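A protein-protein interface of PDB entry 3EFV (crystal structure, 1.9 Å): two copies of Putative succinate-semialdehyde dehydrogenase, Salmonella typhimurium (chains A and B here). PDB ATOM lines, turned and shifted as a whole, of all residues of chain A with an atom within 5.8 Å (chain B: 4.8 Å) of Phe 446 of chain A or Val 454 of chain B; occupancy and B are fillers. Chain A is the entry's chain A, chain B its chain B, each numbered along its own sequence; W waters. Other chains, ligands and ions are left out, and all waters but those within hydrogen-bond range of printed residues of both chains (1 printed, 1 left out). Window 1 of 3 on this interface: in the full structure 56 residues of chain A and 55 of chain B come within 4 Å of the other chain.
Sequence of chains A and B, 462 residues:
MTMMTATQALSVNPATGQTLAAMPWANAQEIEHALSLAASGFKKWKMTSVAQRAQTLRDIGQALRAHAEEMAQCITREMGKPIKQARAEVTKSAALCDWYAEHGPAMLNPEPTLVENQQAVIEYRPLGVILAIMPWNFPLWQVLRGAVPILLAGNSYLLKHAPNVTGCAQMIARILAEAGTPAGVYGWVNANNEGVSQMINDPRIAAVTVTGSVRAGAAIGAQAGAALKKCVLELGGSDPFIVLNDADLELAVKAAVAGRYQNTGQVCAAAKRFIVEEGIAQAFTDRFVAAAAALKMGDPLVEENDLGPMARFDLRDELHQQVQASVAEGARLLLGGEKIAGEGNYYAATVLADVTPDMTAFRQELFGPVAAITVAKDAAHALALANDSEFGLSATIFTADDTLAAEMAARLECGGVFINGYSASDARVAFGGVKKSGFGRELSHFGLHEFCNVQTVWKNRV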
ATOM      1  N   TYR A 100      13.418 -30.520  24.339  1.00  0.00           N
ATOM      2  CA  TYR A 100      14.733 -31.087  24.643  1.00  0.00           C
ATOM      3  C   TYR A 100      14.736 -32.112  25.768  1.00  0.00           C
ATOM      4  O   TYR A 100      15.477 -33.085  25.692  1.00  0.00           O
ATOM      5  CB  TYR A 100      15.782 -30.013  24.919  1.00  0.00           C
ATOM      6  CG  TYR A 100      16.435 -29.520  23.648  1.00  0.00           C
ATOM      7  CD1 TYR A 100      16.127 -28.261  23.129  1.00  0.00           C
ATOM      8  CD2 TYR A 100      17.338 -30.333  22.951  1.00  0.00           C
ATOM      9  CE1 TYR A 100      16.718 -27.808  21.939  1.00  0.00           C
ATOM     10  CE2 TYR A 100      17.951 -29.888  21.767  1.00  0.00           C
ATOM     11  CZ  TYR A 100      17.626 -28.628  21.265  1.00  0.00           C
ATOM     12  OH  TYR A 100      18.222 -28.189  20.098  1.00  0.00           O
ATOM     13  N   CYS A 414      21.800 -19.596   1.837  1.00  0.00           N
ATOM     14  CA  CYS A 414      21.311 -19.322   3.188  1.00  0.00           C
ATOM     15  C   CYS A 414      21.042 -20.634   3.916  1.00  0.00           C
ATOM     16  O   CYS A 414      21.010 -21.698   3.283  1.00  0.00           O
ATOM     17  CB  CYS A 414      20.042 -18.488   3.118  1.00  0.00           C
ATOM     18  SG  CYS A 414      18.769 -19.302   2.233  1.00  0.00           S
ATOM     19  N   GLY A 415      20.864 -20.565   5.232  1.00  0.00           N
ATOM     20  CA  GLY A 415      20.739 -21.765   6.046  1.00  0.00           C
ATOM     21  C   GLY A 415      19.336 -22.290   6.250  1.00  0.00           C
ATOM     22  O   GLY A 415      19.146 -23.338   6.867  1.00  0.00           O
ATOM     23  N   GLY A 416      18.344 -21.583   5.726  1.00  0.00           N
ATOM     24  CA  GLY A 416      16.949 -22.037   5.865  1.00  0.00           C
ATOM     25  C   GLY A 416      16.138 -21.538   4.683  1.00  0.00           C
ATOM     26  O   GLY A 416      16.260 -20.371   4.291  1.00  0.00           O
ATOM     27  N   VAL A 429      14.324 -28.251  13.815  1.00  0.00           N
ATOM     28  CA  VAL A 429      15.156 -27.977  12.633  1.00  0.00           C
ATOM     29  C   VAL A 429      16.345 -27.079  12.952  1.00  0.00           C
ATOM     30  O   VAL A 429      16.372 -26.392  13.981  1.00  0.00           O
ATOM     31  CB  VAL A 429      14.337 -27.419  11.423  1.00  0.00           C
ATOM     32  CG1 VAL A 429      13.151 -28.340  11.096  1.00  0.00           C
ATOM     33  CG2 VAL A 429      13.824 -26.008  11.697  1.00  0.00           C
ATOM     34  N   ALA A 430      17.344 -27.108  12.071  1.00  0.00           N
ATOM     35  CA  ALA A 430      18.555 -26.335  12.252  1.00  0.00           C
ATOM     36  C   ALA A 430      18.249 -24.857  11.995  1.00  0.00           C
ATOM     37  O   ALA A 430      17.433 -24.519  11.116  1.00  0.00           O
ATOM     38  CB  ALA A 430      19.614 -26.809  11.265  1.00  0.00           C
ATOM     39  N   GLY A 432      20.492 -21.081  11.423  1.00  0.00           N
ATOM     40  CA  GLY A 432      21.765 -20.354  11.315  1.00  0.00           C
ATOM     41  C   GLY A 432      22.092 -20.123   9.859  1.00  0.00           C
ATOM     42  O   GLY A 432      21.450 -20.700   8.988  1.00  0.00           O
ATOM     43  N   ARG A 441      25.354 -23.829  13.845  1.00  0.00           N
ATOM     44  CA  ARG A 441      23.911 -24.052  13.791  1.00  0.00           C
ATOM     45  C   ARG A 441      23.346 -24.279  15.196  1.00  0.00           C
ATOM     46  O   ARG A 441      23.990 -24.910  16.057  1.00  0.00           O
ATOM     47  CB  ARG A 441      23.565 -25.270  12.910  1.00  0.00           C
ATOM     48  CG  ARG A 441      23.889 -25.139  11.411  1.00  0.00           C
ATOM     49  CD  ARG A 441      22.967 -24.123  10.741  1.00  0.00           C
ATOM     50  NE  ARG A 441      23.250 -23.883   9.325  1.00  0.00           N
ATOM     51  CZ  ARG A 441      24.051 -22.925   8.860  1.00  0.00           C
ATOM     52  NH1 ARG A 441      24.750 -22.137   9.690  1.00  0.00           N
ATOM     53  NH2 ARG A 441      24.178 -22.778   7.546  1.00  0.00           N
ATOM     54  N   GLU A 442      22.140 -23.761  15.411  1.00  0.00           N
ATOM     55  CA  GLU A 442      21.420 -23.975  16.653  1.00  0.00           C
ATOM     56  C   GLU A 442      20.215 -24.888  16.434  1.00  0.00           C
ATOM     57  O   GLU A 442      19.766 -25.114  15.289  1.00  0.00           O
ATOM     58  CB  GLU A 442      20.974 -22.632  17.231  1.00  0.00           C
ATOM     59  CG  GLU A 442      22.122 -21.851  17.855  1.00  0.00           C
ATOM     60  CD  GLU A 442      21.639 -20.596  18.549  1.00  0.00           C
ATOM     61  OE1 GLU A 442      20.981 -19.759  17.878  1.00  0.00           O
ATOM     62  OE2 GLU A 442      21.894 -20.453  19.759  1.00  0.00           O
ATOM     63  N   LEU A 443      19.713 -25.420  17.544  1.00  0.00           N
ATOM     64  CA  LEU A 443      18.493 -26.220  17.588  1.00  0.00           C
ATOM     65  C   LEU A 443      18.689 -27.622  17.017  1.00  0.00           C
ATOM     66  O   LEU A 443      19.787 -27.972  16.586  1.00  0.00           O
ATOM     67  CB  LEU A 443      17.290 -25.463  16.980  1.00  0.00           C
ATOM     68  CG  LEU A 443      16.950 -24.186  17.784  1.00  0.00           C
ATOM     69  CD1 LEU A 443      15.783 -23.415  17.163  1.00  0.00           C
ATOM     70  CD2 LEU A 443      16.675 -24.506  19.255  1.00  0.00           C
ATOM     71  N   SER A 444      17.623 -28.428  17.063  1.00  0.00           N
ATOM     72  CA  SER A 444      17.692 -29.866  16.781  1.00  0.00           C
ATOM     73  C   SER A 444      18.945 -30.468  17.425  1.00  0.00           C
ATOM     74  O   SER A 444      19.325 -30.057  18.537  1.00  0.00           O
ATOM     75  CB  SER A 444      17.614 -30.111  15.271  1.00  0.00           C
ATOM     76  OG  SER A 444      17.617 -31.510  15.004  1.00  0.00           O
ATOM     77  N   HIS A 445      19.604 -31.425  16.760  1.00  0.00           N
ATOM     78  CA  HIS A 445      20.821 -32.009  17.347  1.00  0.00           C
ATOM     79  C   HIS A 445      22.053 -31.121  17.122  1.00  0.00           C
ATOM     80  O   HIS A 445      23.084 -31.283  17.780  1.00  0.00           O
ATOM     81  CB  HIS A 445      21.062 -33.440  16.844  1.00  0.00           C
ATOM     82  CG  HIS A 445      21.088 -33.573  15.353  1.00  0.00           C
ATOM     83  ND1 HIS A 445      22.237 -33.394  14.613  1.00  0.00           N
ATOM     84  CD2 HIS A 445      20.121 -33.923  14.470  1.00  0.00           C
ATOM     85  CE1 HIS A 445      21.974 -33.615  13.336  1.00  0.00           C
ATOM     86  NE2 HIS A 445      20.696 -33.928  13.221  1.00  0.00           N
ATOM     87  N   PHE A 446      21.936 -30.175  16.196  1.00  0.00           N
ATOM     88  CA  PHE A 446      23.040 -29.254  15.910  1.00  0.00           C
ATOM     89  C   PHE A 446      23.420 -28.384  17.092  1.00  0.00           C
ATOM     90  O   PHE A 446      24.602 -28.298  17.459  1.00  0.00           O
ATOM     91  CB  PHE A 446      22.700 -28.416  14.673  1.00  0.00           C
ATOM     92  CG  PHE A 446      22.282 -29.265  13.509  1.00  0.00           C
ATOM     93  CD1 PHE A 446      23.239 -29.889  12.720  1.00  0.00           C
ATOM     94  CD2 PHE A 446      20.928 -29.495  13.249  1.00  0.00           C
ATOM     95  CE1 PHE A 446      22.860 -30.719  11.646  1.00  0.00           C
ATOM     96  CE2 PHE A 446      20.530 -30.321  12.188  1.00  0.00           C
ATOM     97  CZ  PHE A 446      21.489 -30.931  11.387  1.00  0.00           C
ATOM     98  N   GLY A 447      22.421 -27.757  17.710  1.00  0.00           N
ATOM     99  CA  GLY A 447      22.664 -26.896  18.868  1.00  0.00           C
ATOM    100  C   GLY A 447      23.183 -27.660  20.076  1.00  0.00           C
ATOM    101  O   GLY A 447      23.917 -27.118  20.905  1.00  0.00           O
ATOM    102  N   LEU A 448      22.803 -28.920  20.184  1.00  0.00           N
ATOM    103  CA  LEU A 448      23.320 -29.774  21.258  1.00  0.00           C
ATOM    104  C   LEU A 448      24.784 -30.202  21.016  1.00  0.00           C
ATOM    105  O   LEU A 448      25.609 -30.140  21.927  1.00  0.00           O
ATOM    106  CB  LEU A 448      22.417 -30.999  21.411  1.00  0.00           C
ATOM    107  CG  LEU A 448      22.650 -31.808  22.680  1.00  0.00           C
ATOM    108  CD1 LEU A 448      21.617 -31.460  23.725  1.00  0.00           C
ATOM    109  CD2 LEU A 448      22.504 -33.259  22.290  1.00  0.00           C
ATOM    110  N   HIS A 449      25.118 -30.616  19.791  1.00  0.00           N
ATOM    111  CA  HIS A 449      26.469 -31.111  19.504  1.00  0.00           C
ATOM    112  C   HIS A 449      27.533 -30.027  19.266  1.00  0.00           C
ATOM    113  O   HIS A 449      28.726 -30.315  19.374  1.00  0.00           O
ATOM    114  CB  HIS A 449      26.441 -32.091  18.317  1.00  0.00           C
ATOM    115  CG  HIS A 449      25.667 -33.343  18.588  1.00  0.00           C
ATOM    116  ND1 HIS A 449      25.107 -34.104  17.587  1.00  0.00           N
ATOM    117  CD2 HIS A 449      25.359 -33.968  19.749  1.00  0.00           C
ATOM    118  CE1 HIS A 449      24.498 -35.150  18.117  1.00  0.00           C
ATOM    119  NE2 HIS A 449      24.635 -35.093  19.427  1.00  0.00           N
ATOM    120  N   GLU A 450      27.124 -28.793  18.957  1.00  0.00           N
ATOM    121  CA  GLU A 450      28.094 -27.693  18.729  1.00  0.00           C
ATOM    122  C   GLU A 450      28.996 -27.504  19.930  1.00  0.00           C
ATOM    123  O   GLU A 450      30.173 -27.147  19.767  1.00  0.00           O
ATOM    124  CB  GLU A 450      27.395 -26.362  18.417  1.00  0.00           C
ATOM    125  CG  GLU A 450      26.807 -26.237  17.003  1.00  0.00           C
ATOM    126  CD  GLU A 450      27.826 -25.856  15.910  1.00  0.00           C
ATOM    127  OE1 GLU A 450      29.035 -25.664  16.197  1.00  0.00           O
ATOM    128  OE2 GLU A 450      27.407 -25.745  14.748  1.00  0.00           O
ATOM    129  N   PHE A 451      28.467 -27.755  21.131  1.00  0.00           N
ATOM    130  CA  PHE A 451      29.252 -27.562  22.350  1.00  0.00           C
ATOM    131  C   PHE A 451      29.522 -28.867  23.104  1.00  0.00           C
ATOM    132  O   PHE A 451      29.584 -28.898  24.346  1.00  0.00           O
ATOM    133  CB  PHE A 451      28.637 -26.454  23.232  1.00  0.00           C
ATOM    134  CG  PHE A 451      28.577 -25.130  22.525  1.00  0.00           C
ATOM    135  CD1 PHE A 451      29.729 -24.392  22.324  1.00  0.00           C
ATOM    136  CD2 PHE A 451      27.393 -24.673  21.993  1.00  0.00           C
ATOM    137  CE1 PHE A 451      29.690 -23.179  21.627  1.00  0.00           C
ATOM    138  CE2 PHE A 451      27.342 -23.459  21.291  1.00  0.00           C
ATOM    139  CZ  PHE A 451      28.489 -22.725  21.117  1.00  0.00           C
ATOM    140  N   GLU B 111      18.403 -35.295   5.816  1.00  0.00           N
ATOM    141  CA  GLU B 111      17.909 -35.885   7.055  1.00  0.00           C
ATOM    142  C   GLU B 111      16.429 -35.616   7.187  1.00  0.00           C
ATOM    143  O   GLU B 111      16.010 -34.468   7.009  1.00  0.00           O
ATOM    144  CB  GLU B 111      18.540 -35.196   8.272  1.00  0.00           C
ATOM    145  CG  GLU B 111      19.833 -35.734   8.746  1.00  0.00           C
ATOM    146  CD  GLU B 111      20.359 -34.982   9.969  1.00  0.00           C
ATOM    147  OE1 GLU B 111      19.548 -34.409  10.755  1.00  0.00           O
ATOM    148  OE2 GLU B 111      21.598 -34.951  10.131  1.00  0.00           O
ATOM    149  N   ILE B 122      16.619 -31.635   6.401  1.00  0.00           N
ATOM    150  CA  ILE B 122      17.884 -30.921   6.509  1.00  0.00           C
ATOM    151  C   ILE B 122      18.754 -31.364   5.348  1.00  0.00           C
ATOM    152  O   ILE B 122      18.960 -32.581   5.155  1.00  0.00           O
ATOM    153  CB  ILE B 122      18.613 -31.285   7.816  1.00  0.00           C
ATOM    154  CG1 ILE B 122      17.692 -31.156   9.045  1.00  0.00           C
ATOM    155  CG2 ILE B 122      19.933 -30.476   7.945  1.00  0.00           C
ATOM    156  CD1 ILE B 122      17.165 -29.722   9.337  1.00  0.00           C
ATOM    157  N   GLU B 123      19.255 -30.408   4.569  1.00  0.00           N
ATOM    158  CA  GLU B 123      20.115 -30.740   3.420  1.00  0.00           C
ATOM    159  C   GLU B 123      21.529 -30.326   3.740  1.00  0.00           C
ATOM    160  O   GLU B 123      21.715 -29.348   4.465  1.00  0.00           O
ATOM    161  CB  GLU B 123      19.653 -29.970   2.179  1.00  0.00           C
ATOM    162  CG  GLU B 123      18.253 -30.359   1.711  1.00  0.00           C
ATOM    163  CD  GLU B 123      18.245 -31.554   0.756  1.00  0.00           C
ATOM    164  OE1 GLU B 123      19.277 -32.261   0.616  1.00  0.00           O
ATOM    165  OE2 GLU B 123      17.194 -31.769   0.131  1.00  0.00           O
ATOM    166  N   TYR B 124      22.521 -31.033   3.182  1.00  0.00           N
ATOM    167  CA  TYR B 124      23.927 -30.684   3.406  1.00  0.00           C
ATOM    168  C   TYR B 124      24.465 -30.079   2.115  1.00  0.00           C
ATOM    169  O   TYR B 124      24.851 -30.813   1.184  1.00  0.00           O
ATOM    170  CB  TYR B 124      24.748 -31.908   3.865  1.00  0.00           C
ATOM    171  CG  TYR B 124      24.363 -32.405   5.243  1.00  0.00           C
ATOM    172  CD1 TYR B 124      24.962 -31.883   6.386  1.00  0.00           C
ATOM    173  CD2 TYR B 124      23.367 -33.376   5.404  1.00  0.00           C
ATOM    174  CE1 TYR B 124      24.591 -32.319   7.662  1.00  0.00           C
ATOM    175  CE2 TYR B 124      22.986 -33.817   6.671  1.00  0.00           C
ATOM    176  CZ  TYR B 124      23.603 -33.287   7.788  1.00  0.00           C
ATOM    177  OH  TYR B 124      23.237 -33.719   9.047  1.00  0.00           O
ATOM    178  N   CYS B 452      29.957 -27.980   5.334  1.00  0.00           N
ATOM    179  CA  CYS B 452      28.678 -27.890   4.657  1.00  0.00           C
ATOM    180  C   CYS B 452      27.877 -26.706   5.178  1.00  0.00           C
ATOM    181  O   CYS B 452      27.993 -26.322   6.358  1.00  0.00           O
ATOM    182  CB  CYS B 452      27.854 -29.149   4.884  1.00  0.00           C
ATOM    183  SG  CYS B 452      28.494 -30.566   3.908  1.00  0.00           S
ATOM    184  N   ASN B 453      27.066 -26.146   4.294  1.00  0.00           N
ATOM    185  CA  ASN B 453      25.957 -25.299   4.705  1.00  0.00           C
ATOM    186  C   ASN B 453      24.792 -26.234   5.069  1.00  0.00           C
ATOM    187  O   ASN B 453      24.156 -26.822   4.205  1.00  0.00           O
ATOM    188  CB  ASN B 453      25.584 -24.320   3.571  1.00  0.00           C
ATOM    189  CG  ASN B 453      24.224 -23.683   3.781  1.00  0.00           C
ATOM    190  OD1 ASN B 453      23.723 -23.628   4.904  1.00  0.00           O
ATOM    191  ND2 ASN B 453      23.612 -23.217   2.696  1.00  0.00           N
ATOM    192  N   VAL B 454      24.558 -26.409   6.364  1.00  0.00           N
ATOM    193  CA  VAL B 454      23.474 -27.248   6.848  1.00  0.00           C
ATOM    194  C   VAL B 454      22.191 -26.412   6.695  1.00  0.00           C
ATOM    195  O   VAL B 454      22.031 -25.370   7.349  1.00  0.00           O
ATOM    196  CB  VAL B 454      23.738 -27.651   8.316  1.00  0.00           C
ATOM    197  CG1 VAL B 454      22.476 -28.237   8.995  1.00  0.00           C
ATOM    198  CG2 VAL B 454      24.925 -28.628   8.397  1.00  0.00           C
ATOM    199  N   GLN B 455      21.297 -26.844   5.813  1.00  0.00           N
ATOM    200  CA  GLN B 455      20.194 -25.991   5.383  1.00  0.00           C
ATOM    201  C   GLN B 455      18.860 -26.689   5.648  1.00  0.00           C
ATOM    202  O   GLN B 455      18.615 -27.791   5.135  1.00  0.00           O
ATOM    203  CB  GLN B 455      20.320 -25.689   3.878  1.00  0.00           C
ATOM    204  CG  GLN B 455      19.267 -24.691   3.318  1.00  0.00           C
ATOM    205  CD  GLN B 455      19.252 -24.657   1.816  1.00  0.00           C
ATOM    206  OE1 GLN B 455      18.885 -25.648   1.180  1.00  0.00           O
ATOM    207  NE2 GLN B 455      19.650 -23.521   1.229  1.00  0.00           N
ATOM    208  N   THR B 456      18.015 -26.057   6.456  1.00  0.00           N
ATOM    209  CA  THR B 456      16.645 -26.497   6.624  1.00  0.00           C
ATOM    210  C   THR B 456      15.826 -26.147   5.366  1.00  0.00           C
ATOM    211  O   THR B 456      15.892 -25.016   4.884  1.00  0.00           O
ATOM    212  CB  THR B 456      16.033 -25.824   7.872  1.00  0.00           C
ATOM    213  OG1 THR B 456      16.740 -26.307   9.014  1.00  0.00           O
ATOM    214  CG2 THR B 456      14.535 -26.173   8.012  1.00  0.00           C
HETATM  215  O   HOH W   1      26.505 -25.258   8.349  1.00  0.00           O
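Of the 18 printed residues of chain A, 8 touch a printed residue of chain B. Printed residues of chain A that touch a printed residue of chain B: Cys 414, Gly 415, Gly 416, Val 429, Ala 430, Arg 441, His 445 and Phe 446. Among the printed residues, no Asp or Glu carboxylate lies within 4 Å of a Lys or Arg side-chain nitrogen of the other chain.
The backbone carbonyl oxygen (O) of Cys 414 of chain A sits at hydrogen-bond distance from the side-chain amide nitrogen (ND2) of Asn 453 of chain B (3.1 Å). The backbone carbonyl oxygen of Cys 414 of chain A lies within hydrogen-bond range of the side-chain amide nitrogen of Gln 455 of chain B. N of Thr 456 of chain B lies within hydrogen-bond range of O of Gly 415 of chain A (3.0 Å). The backbone carbonyl oxygen (O) of Ala 430 of chain A lies within hydrogen-bond range of the side-chain hydroxyl (OG1) of Thr 456 of chain B. The side-chain amide oxygen (OD1) of Asn 453 of chain B lies within hydrogen-bond range of the guanidinium group (NH2) of Arg 441 of chain A (2.8 Å). NE of Arg 441 of chain A sits at hydrogen-bond distance from O of Val 454 of chain B. A ring nitrogen (NE2) of His 445 of chain A is in hydrogen-bond range of the side-chain carboxylate of Glu 111 of chain B, 2.8 Å away.
Water W1 lies within hydrogen-bond range of the backbone carbonyl oxygen (O) of Cys 452 of chain B (2.7 Å), the backbone NH (N) of Val 454 of chain B (3.0 Å) and the guanidinium group (NH2) of Arg 441 of chain A (3.5 Å).
The side-chain sulfur (SG) of Cys 414 of chain A lies within hydrogen-bond range of the backbone carbonyl oxygen (O) of Gly 416 of chain A (3.4 Å). OE2 of Glu 450 of chain A is in hydrogen-bond range of N of Arg 441 of chain A (2.9 Å). ND1 of His 449 of chain A sits close to O of His 445 of chain A. The backbone NH (N) of Glu 111 of chain B sits at hydrogen-bond distance from the backbone carbonyl oxygen (O) of Ile 122 of chain B (2.8 Å). N of Glu 123 of chain B is in hydrogen-bond range of O of Gln 455 of chain B (2.8 Å).
Printed residues of chain B within 4 Å of Phe 446 of chain A: Ile 122 (3.8 Å), Tyr 124 (3.99 Å) and Val 454 (3.7 Å). Val 454 of chain B touches just these residues of chain A: Gly 415, Ala 430, Arg 441 and Phe 446. Printed residues of chain A within 4 Å of Tyr 124 of chain B: Phe 446 (3.99 Å). Of the printed residues of chain B, Gly 416 of chain A touches Thr 456 (3.3 Å). Printed residues of chain B within 4 Å of Gly 415 of chain A: Asn 453 (3.7 Å), Val 454 (3.6 Å), Gln 455 (3.2 Å) and Thr 456 (3.0 Å). Of the printed residues of chain B, Ala 430 of chain A touches Ile 122 (3.8 Å), Val 454 (3.9 Å) and Thr 456 (2.8 Å). Of the printed residues of chain A, Gln 455 of chain B touches Cys 414 (3.1 Å) and Gly 415 (3.2 Å). The nearest residue of chain A that does not touch Val 454 of chain B is Gly 432 of chain A (5.0 Å). The nearest printed residue of chain B that does not touch Gly 415 of chain A is Glu 123 of chain B (7.0 Å).
Asn 453 of chain B touches Gly 415 of chain A. Gly 415 of chain A touches Val 454 of chain B. Gly 415 of chain A touches Gln 455 of chain B (O to CA, 3.2 Å). Gly 416 of chain A touches Thr 456 of chain B (CA to O, 3.3 Å). Val 429 of chain A touches Thr 456 of chain B (CB to OG1, 3.6 Å). Ala 430 of chain A touches Ile 122 of chain B (N to CD1, 3.8 Å). Val 454 of chain B touches Ala 430 of chain A. Ile 122 of chain B touches Phe 446 of chain A (CG2 to CZ, 3.8 Å). Tyr 124 of chain B touches Phe 446 of chain A. Val 454 of chain B touches Phe 446 of chain A.
No position is printed for both chains. Of the 17 pairs that touch across the chains among the printed residues, none has its exchanged pair printed and touching as well.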
